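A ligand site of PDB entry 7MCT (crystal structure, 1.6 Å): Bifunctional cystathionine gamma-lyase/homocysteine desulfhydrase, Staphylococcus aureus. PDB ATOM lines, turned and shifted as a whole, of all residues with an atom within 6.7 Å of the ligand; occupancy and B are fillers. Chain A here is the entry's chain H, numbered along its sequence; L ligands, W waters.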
ATOM      1  N   SER A  96     -16.399 -29.092  28.240  1.00  0.00           N
ATOM      2  CA  SER A  96     -17.497 -29.940  28.675  1.00  0.00           C
ATOM      3  C   SER A  96     -18.807 -29.581  28.008  1.00  0.00           C
ATOM      4  O   SER A  96     -19.648 -30.461  27.767  1.00  0.00           O
ATOM      5  CB  SER A  96     -17.654 -29.864  30.205  1.00  0.00           C
ATOM      6  OG  SER A  96     -17.822 -28.520  30.626  1.00  0.00           O
ATOM      7  N   ASP A  97     -19.010 -28.304  27.708  1.00  0.00           N
ATOM      8  CA  ASP A  97     -20.299 -27.807  27.231  1.00  0.00           C
ATOM      9  C   ASP A  97     -20.240 -27.400  25.757  1.00  0.00           C
ATOM     10  O   ASP A  97     -20.854 -26.422  25.344  1.00  0.00           O
ATOM     11  CB  ASP A  97     -20.767 -26.634  28.077  1.00  0.00           C
ATOM     12  CG  ASP A  97     -19.741 -25.528  28.182  1.00  0.00           C
ATOM     13  OD1 ASP A  97     -18.613 -25.695  27.669  1.00  0.00           O
ATOM     14  OD2 ASP A  97     -20.051 -24.473  28.788  1.00  0.00           O
ATOM     15  N   VAL A  98     -19.510 -28.177  24.950  1.00  0.00           N
ATOM     16  CA  VAL A  98     -19.354 -27.856  23.527  1.00  0.00           C
ATOM     17  C   VAL A  98     -20.718 -27.827  22.818  1.00  0.00           C
ATOM     18  O   VAL A  98     -21.695 -28.440  23.260  1.00  0.00           O
ATOM     19  CB  VAL A  98     -18.397 -28.883  22.896  1.00  0.00           C
ATOM     20  CG1 VAL A  98     -19.123 -30.184  22.562  1.00  0.00           C
ATOM     21  CG2 VAL A  98     -17.716 -28.296  21.663  1.00  0.00           C
ATOM     22  N   TYR A  99     -20.766 -27.074  21.711  1.00  0.00           N
ATOM     23  CA  TYR A  99     -21.966 -26.948  20.902  1.00  0.00           C
ATOM     24  C   TYR A  99     -22.606 -28.308  20.629  1.00  0.00           C
ATOM     25  O   TYR A  99     -21.915 -29.291  20.348  1.00  0.00           O
ATOM     26  CB  TYR A  99     -21.606 -26.252  19.591  1.00  0.00           C
ATOM     27  CG  TYR A  99     -22.683 -26.259  18.527  1.00  0.00           C
ATOM     28  CD1 TYR A  99     -23.859 -25.545  18.701  1.00  0.00           C
ATOM     29  CD2 TYR A  99     -22.502 -26.957  17.340  1.00  0.00           C
ATOM     30  CE1 TYR A  99     -24.835 -25.534  17.724  1.00  0.00           C
ATOM     31  CE2 TYR A  99     -23.477 -26.963  16.357  1.00  0.00           C
ATOM     32  CZ  TYR A  99     -24.634 -26.250  16.555  1.00  0.00           C
ATOM     33  OH  TYR A  99     -25.602 -26.250  15.575  1.00  0.00           O
ATOM     34  N   GLY A 100     -23.941 -28.360  20.717  1.00  0.00           N
ATOM     35  CA  GLY A 100     -24.646 -29.619  20.587  1.00  0.00           C
ATOM     36  C   GLY A 100     -24.354 -30.356  19.295  1.00  0.00           C
ATOM     37  O   GLY A 100     -24.241 -31.586  19.284  1.00  0.00           O
ATOM     38  N   GLY A 101     -24.234 -29.624  18.184  1.00  0.00           N
ATOM     39  CA  GLY A 101     -23.878 -30.274  16.934  1.00  0.00           C
ATOM     40  C   GLY A 101     -22.489 -30.897  16.969  1.00  0.00           C
ATOM     41  O   GLY A 101     -22.268 -31.970  16.404  1.00  0.00           O
ATOM     42  N   TYR A 103     -21.007 -31.968  19.769  1.00  0.00           N
ATOM     43  CA  TYR A 103     -21.168 -33.136  20.631  1.00  0.00           C
ATOM     44  C   TYR A 103     -21.761 -34.311  19.855  1.00  0.00           C
ATOM     45  O   TYR A 103     -21.287 -35.443  19.966  1.00  0.00           O
ATOM     46  CB  TYR A 103     -22.050 -32.775  21.832  1.00  0.00           C
ATOM     47  CG  TYR A 103     -22.337 -33.960  22.726  1.00  0.00           C
ATOM     48  CD1 TYR A 103     -21.443 -34.325  23.726  1.00  0.00           C
ATOM     49  CD2 TYR A 103     -23.485 -34.728  22.557  1.00  0.00           C
ATOM     50  CE1 TYR A 103     -21.698 -35.415  24.542  1.00  0.00           C
ATOM     51  CE2 TYR A 103     -23.743 -35.826  23.363  1.00  0.00           C
ATOM     52  CZ  TYR A 103     -22.845 -36.156  24.352  1.00  0.00           C
ATOM     53  OH  TYR A 103     -23.087 -37.244  25.162  1.00  0.00           O
ATOM     54  N   ARG A 104     -22.814 -34.044  19.066  1.00  0.00           N
ATOM     55  CA  ARG A 104     -23.481 -35.104  18.302  1.00  0.00           C
ATOM     56  C   ARG A 104     -22.555 -35.701  17.262  1.00  0.00           C
ATOM     57  O   ARG A 104     -22.465 -36.929  17.116  1.00  0.00           O
ATOM     58  CB  ARG A 104     -24.723 -34.560  17.605  1.00  0.00           C
ATOM     59  CG  ARG A 104     -25.931 -34.291  18.470  1.00  0.00           C
ATOM     60  CD  ARG A 104     -27.137 -33.915  17.590  1.00  0.00           C
ATOM     61  NE  ARG A 104     -26.882 -32.741  16.743  1.00  0.00           N
ATOM     62  CZ  ARG A 104     -26.708 -32.772  15.425  1.00  0.00           C
ATOM     63  NH1 ARG A 104     -26.782 -33.927  14.769  1.00  0.00           N
ATOM     64  NH2 ARG A 104     -26.473 -31.648  14.754  1.00  0.00           N
ATOM     65  N   THR A 107     -19.880 -37.843  19.182  1.00  0.00           N
ATOM     66  CA  THR A 107     -20.308 -39.021  19.943  1.00  0.00           C
ATOM     67  C   THR A 107     -21.197 -39.974  19.157  1.00  0.00           C
ATOM     68  O   THR A 107     -21.340 -41.134  19.567  1.00  0.00           O
ATOM     69  CB  THR A 107     -21.034 -38.614  21.229  1.00  0.00           C
ATOM     70  OG1 THR A 107     -22.206 -37.835  20.909  1.00  0.00           O
ATOM     71  CG2 THR A 107     -20.114 -37.815  22.151  1.00  0.00           C
ATOM     72  N   ASN A 146     -21.609 -22.079  24.835  1.00  0.00           N
ATOM     73  CA  ASN A 146     -23.054 -21.895  24.773  1.00  0.00           C
ATOM     74  C   ASN A 146     -23.777 -22.887  25.684  1.00  0.00           C
ATOM     75  O   ASN A 146     -23.378 -24.063  25.731  1.00  0.00           O
ATOM     76  CB  ASN A 146     -23.548 -22.076  23.333  1.00  0.00           C
ATOM     77  CG  ASN A 146     -25.035 -21.862  23.211  1.00  0.00           C
ATOM     78  OD1 ASN A 146     -25.517 -20.727  23.325  1.00  0.00           O
ATOM     79  ND2 ASN A 146     -25.778 -22.936  22.977  1.00  0.00           N
ATOM     80  N   PRO A 147     -24.831 -22.468  26.401  1.00  0.00           N
ATOM     81  CA  PRO A 147     -25.400 -21.121  26.507  1.00  0.00           C
ATOM     82  C   PRO A 147     -24.969 -20.366  27.758  1.00  0.00           C
ATOM     83  O   PRO A 147     -25.505 -19.295  28.033  1.00  0.00           O
ATOM     84  CB  PRO A 147     -26.907 -21.393  26.554  1.00  0.00           C
ATOM     85  CG  PRO A 147     -26.981 -22.664  27.371  1.00  0.00           C
ATOM     86  CD  PRO A 147     -25.732 -23.468  27.006  1.00  0.00           C
ATOM     87  N   MET A 337     -35.548 -25.999  23.400  1.00  0.00           N
ATOM     88  CA  MET A 337     -35.198 -25.952  21.985  1.00  0.00           C
ATOM     89  C   MET A 337     -33.924 -26.698  21.649  1.00  0.00           C
ATOM     90  O   MET A 337     -33.905 -27.487  20.705  1.00  0.00           O
ATOM     91  CB  MET A 337     -35.091 -24.490  21.527  1.00  0.00           C
ATOM     92  CG  MET A 337     -36.444 -23.795  21.534  1.00  0.00           C
ATOM     93  SD  MET A 337     -36.393 -22.012  21.288  1.00  0.00           S
ATOM     94  CE  MET A 337     -35.673 -21.871  19.650  1.00  0.00           C
ATOM     95  N   THR A 338     -32.855 -26.474  22.397  1.00  0.00           N
ATOM     96  CA  THR A 338     -31.578 -27.116  22.097  1.00  0.00           C
ATOM     97  C   THR A 338     -31.240 -28.242  23.049  1.00  0.00           C
ATOM     98  O   THR A 338     -30.593 -29.209  22.628  1.00  0.00           O
ATOM     99  CB  THR A 338     -30.450 -26.075  22.103  1.00  0.00           C
ATOM    100  OG1 THR A 338     -30.411 -25.397  23.364  1.00  0.00           O
ATOM    101  CG2 THR A 338     -30.661 -25.062  21.000  1.00  0.00           C
ATOM    102  N   HIS A 339     -31.680 -28.182  24.300  1.00  0.00           N
ATOM    103  CA  HIS A 339     -31.333 -29.170  25.315  1.00  0.00           C
ATOM    104  C   HIS A 339     -32.527 -30.033  25.725  1.00  0.00           C
ATOM    105  O   HIS A 339     -32.509 -30.625  26.804  1.00  0.00           O
ATOM    106  CB  HIS A 339     -30.726 -28.489  26.537  1.00  0.00           C
ATOM    107  CG  HIS A 339     -29.410 -27.826  26.283  1.00  0.00           C
ATOM    108  ND1 HIS A 339     -29.285 -26.708  25.491  1.00  0.00           N
ATOM    109  CD2 HIS A 339     -28.166 -28.111  26.740  1.00  0.00           C
ATOM    110  CE1 HIS A 339     -28.014 -26.341  25.454  1.00  0.00           C
ATOM    111  NE2 HIS A 339     -27.322 -27.169  26.208  1.00  0.00           N
ATOM    112  N   ALA A 340     -33.554 -30.126  24.867  1.00  0.00           N
ATOM    113  CA  ALA A 340     -34.826 -30.713  25.300  1.00  0.00           C
ATOM    114  C   ALA A 340     -34.731 -32.214  25.524  1.00  0.00           C
ATOM    115  O   ALA A 340     -35.498 -32.763  26.330  1.00  0.00           O
ATOM    116  CB  ALA A 340     -35.905 -30.397  24.272  1.00  0.00           C
ATOM    117  N   SER A 341     -33.827 -32.913  24.837  1.00  0.00           N
ATOM    118  CA  SER A 341     -33.769 -34.365  24.986  1.00  0.00           C
ATOM    119  C   SER A 341     -33.047 -34.798  26.252  1.00  0.00           C
ATOM    120  O   SER A 341     -33.082 -35.989  26.589  1.00  0.00           O
ATOM    121  CB  SER A 341     -33.120 -34.992  23.762  1.00  0.00           C
ATOM    122  OG  SER A 341     -31.825 -34.458  23.544  1.00  0.00           O
ATOM    123  N   ILE A 342     -32.385 -33.879  26.945  1.00  0.00           N
ATOM    124  CA  ILE A 342     -31.682 -34.169  28.183  1.00  0.00           C
ATOM    125  C   ILE A 342     -32.688 -34.227  29.323  1.00  0.00           C
ATOM    126  O   ILE A 342     -33.606 -33.385  29.392  1.00  0.00           O
ATOM    127  CB  ILE A 342     -30.591 -33.127  28.435  1.00  0.00           C
ATOM    128  CG1 ILE A 342     -29.573 -33.192  27.298  1.00  0.00           C
ATOM    129  CG2 ILE A 342     -29.948 -33.357  29.810  1.00  0.00           C
ATOM    130  CD1 ILE A 342     -28.929 -31.879  27.047  1.00  0.00           C
ATOM    131  N   PRO A 343     -32.598 -35.225  30.206  1.00  0.00           N
ATOM    132  CA  PRO A 343     -33.525 -35.317  31.331  1.00  0.00           C
ATOM    133  C   PRO A 343     -33.566 -34.026  32.124  1.00  0.00           C
ATOM    134  O   PRO A 343     -32.551 -33.339  32.294  1.00  0.00           O
ATOM    135  CB  PRO A 343     -32.943 -36.480  32.158  1.00  0.00           C
ATOM    136  CG  PRO A 343     -32.408 -37.398  31.074  1.00  0.00           C
ATOM    137  CD  PRO A 343     -31.694 -36.395  30.166  1.00  0.00           C
ATOM    138  N   ILE A 346     -31.167 -33.512  35.007  1.00  0.00           N
ATOM    139  CA  ILE A 346     -29.799 -33.285  34.569  1.00  0.00           C
ATOM    140  C   ILE A 346     -29.654 -31.876  33.983  1.00  0.00           C
ATOM    141  O   ILE A 346     -28.648 -31.188  34.221  1.00  0.00           O
ATOM    142  CB  ILE A 346     -29.380 -34.377  33.568  1.00  0.00           C
ATOM    143  CG1 ILE A 346     -29.190 -35.703  34.315  1.00  0.00           C
ATOM    144  CG2 ILE A 346     -28.083 -34.004  32.854  1.00  0.00           C
ATOM    145  CD1 ILE A 346     -29.524 -36.934  33.490  1.00  0.00           C
ATOM    146  N   ARG A 347     -30.658 -31.413  33.235  1.00  0.00           N
ATOM    147  CA  ARG A 347     -30.670 -30.025  32.797  1.00  0.00           C
ATOM    148  C   ARG A 347     -30.517 -29.082  33.977  1.00  0.00           C
ATOM    149  O   ARG A 347     -29.667 -28.179  33.972  1.00  0.00           O
ATOM    150  CB  ARG A 347     -31.960 -29.706  32.035  1.00  0.00           C
ATOM    151  CG  ARG A 347     -32.008 -30.274  30.631  1.00  0.00           C
ATOM    152  CD  ARG A 347     -32.964 -29.479  29.775  1.00  0.00           C
ATOM    153  NE  ARG A 347     -34.278 -29.363  30.395  1.00  0.00           N
ATOM    154  CZ  ARG A 347     -35.291 -30.194  30.183  1.00  0.00           C
ATOM    155  NH1 ARG A 347     -35.139 -31.217  29.354  1.00  0.00           N
ATOM    156  NH2 ARG A 347     -36.455 -29.998  30.786  1.00  0.00           N
ATOM    157  N   GLU A 350     -27.136 -28.963  35.413  1.00  0.00           N
ATOM    158  CA  GLU A 350     -26.178 -28.259  34.575  1.00  0.00           C
ATOM    159  C   GLU A 350     -26.455 -26.759  34.489  1.00  0.00           C
ATOM    160  O   GLU A 350     -25.720 -26.051  33.788  1.00  0.00           O
ATOM    161  CB  GLU A 350     -26.194 -28.858  33.178  1.00  0.00           C
ATOM    162  CG  GLU A 350     -25.688 -30.281  33.124  1.00  0.00           C
ATOM    163  CD  GLU A 350     -24.198 -30.379  33.338  1.00  0.00           C
ATOM    164  OE1 GLU A 350     -23.483 -29.428  32.959  1.00  0.00           O
ATOM    165  OE2 GLU A 350     -23.741 -31.395  33.893  1.00  0.00           O
ATOM    166  N   GLY A 351     -27.480 -26.258  35.168  1.00  0.00           N
ATOM    167  CA  GLY A 351     -27.821 -24.850  35.091  1.00  0.00           C
ATOM    168  C   GLY A 351     -28.716 -24.487  33.934  1.00  0.00           C
ATOM    169  O   GLY A 351     -29.016 -23.290  33.765  1.00  0.00           O
ATOM    170  N   ILE A 352     -29.144 -25.454  33.127  1.00  0.00           N
ATOM    171  CA  ILE A 352     -30.074 -25.195  32.036  1.00  0.00           C
ATOM    172  C   ILE A 352     -31.489 -25.280  32.587  1.00  0.00           C
ATOM    173  O   ILE A 352     -32.229 -26.240  32.325  1.00  0.00           O
ATOM    174  CB  ILE A 352     -29.867 -26.188  30.876  1.00  0.00           C
ATOM    175  CG1 ILE A 352     -28.383 -26.327  30.544  1.00  0.00           C
ATOM    176  CG2 ILE A 352     -30.631 -25.739  29.629  1.00  0.00           C
ATOM    177  CD1 ILE A 352     -27.719 -25.012  30.182  1.00  0.00           C
HETATM  178  C1  LIG L   1     -24.635 -31.376  24.904  1.00  0.00           C
HETATM  179  C2  LIG L   1     -25.917 -30.997  24.185  1.00  0.00           C
HETATM  180  C3  LIG L   1     -27.104 -28.963  23.583  1.00  0.00           C
HETATM  181  C4  LIG L   1     -27.352 -28.443  22.182  1.00  0.00           C
HETATM  182  C5  LIG L   1     -24.484 -33.811  25.605  1.00  0.00           C
HETATM  183  C6  LIG L   1     -24.773 -34.564  26.736  1.00  0.00           C
HETATM  184  C7  LIG L   1     -25.770 -33.811  29.046  1.00  0.00           C
HETATM  185  C8  LIG L   1     -26.230 -32.688  29.734  1.00  0.00           C
HETATM  186  C9  LIG L   1     -26.209 -31.444  29.114  1.00  0.00           C
HETATM  187  C10 LIG L   1     -25.753 -31.308  27.847  1.00  0.00           C
HETATM  188  C11 LIG L   1     -25.305 -32.413  27.158  1.00  0.00           C
HETATM  189  C12 LIG L   1     -25.302 -33.673  27.737  1.00  0.00           C
HETATM  190  N1  LIG L   1     -24.808 -32.498  25.864  1.00  0.00           N
HETATM  191  N2  LIG L   1     -25.919 -29.796  23.616  1.00  0.00           N
HETATM  192  O1  LIG L   1     -26.866 -31.766  24.156  1.00  0.00           O
HETATM  193  O2  LIG L   1     -26.872 -27.339  21.841  1.00  0.00           O
HETATM  194  O3  LIG L   1     -28.029 -29.143  21.399  1.00  0.00           O
HETATM  195 BR1  LIG L   1     -26.821 -29.896  30.005  1.00  0.00          BR
HETATM  196  O   HOH W   1     -28.489 -28.497  19.114  1.00  0.00           O
HETATM  197  O   HOH W   2     -27.258 -34.458  22.144  1.00  0.00           O
HETATM  198  O   HOH W   3     -21.608 -30.612  25.207  1.00  0.00           O
HETATM  199  O   HOH W   4     -27.544 -24.684  20.008  1.00  0.00           O
HETATM  200  O   HOH W   5     -25.011 -25.716  22.646  1.00  0.00           O
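Residues that only touch the ligand: Tyr 103 (3.1 Å), His 339 (3.2 Å), Ile 342 (3.3 Å), Ile 346 (3.9 Å), Glu 350 (3.3 Å) and Ile 352 (3.9 Å).
OG1 of Thr 338 is in hydrogen-bond range of ND1 of His 339 (2.7 Å).
O of Tyr 103 sits at hydrogen-bond distance from OG1 of Thr 107 (2.7 Å).
The backbone carbonyl oxygen (O) of Ile 342 sits at hydrogen-bond distance from the guanidinium group (NH1) of Arg 347 (2.7 Å).
The backbone NH of Ile 352 is in hydrogen-bond range of the backbone carbonyl oxygen of Arg 347 (2.9 Å).
Water W5 lies within hydrogen-bond range of an oxygen (O2) of the ligand (2.6 Å), the side-chain amide nitrogen (ND2) of Asn 146 (2.9 Å) and the backbone NH (N) of Gly 100 (3.4 Å).
O of Thr 338 sits close to O3 of the ligand (2.8 Å).
N of Gly 100 lies within hydrogen-bond range of O2 of the ligand.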
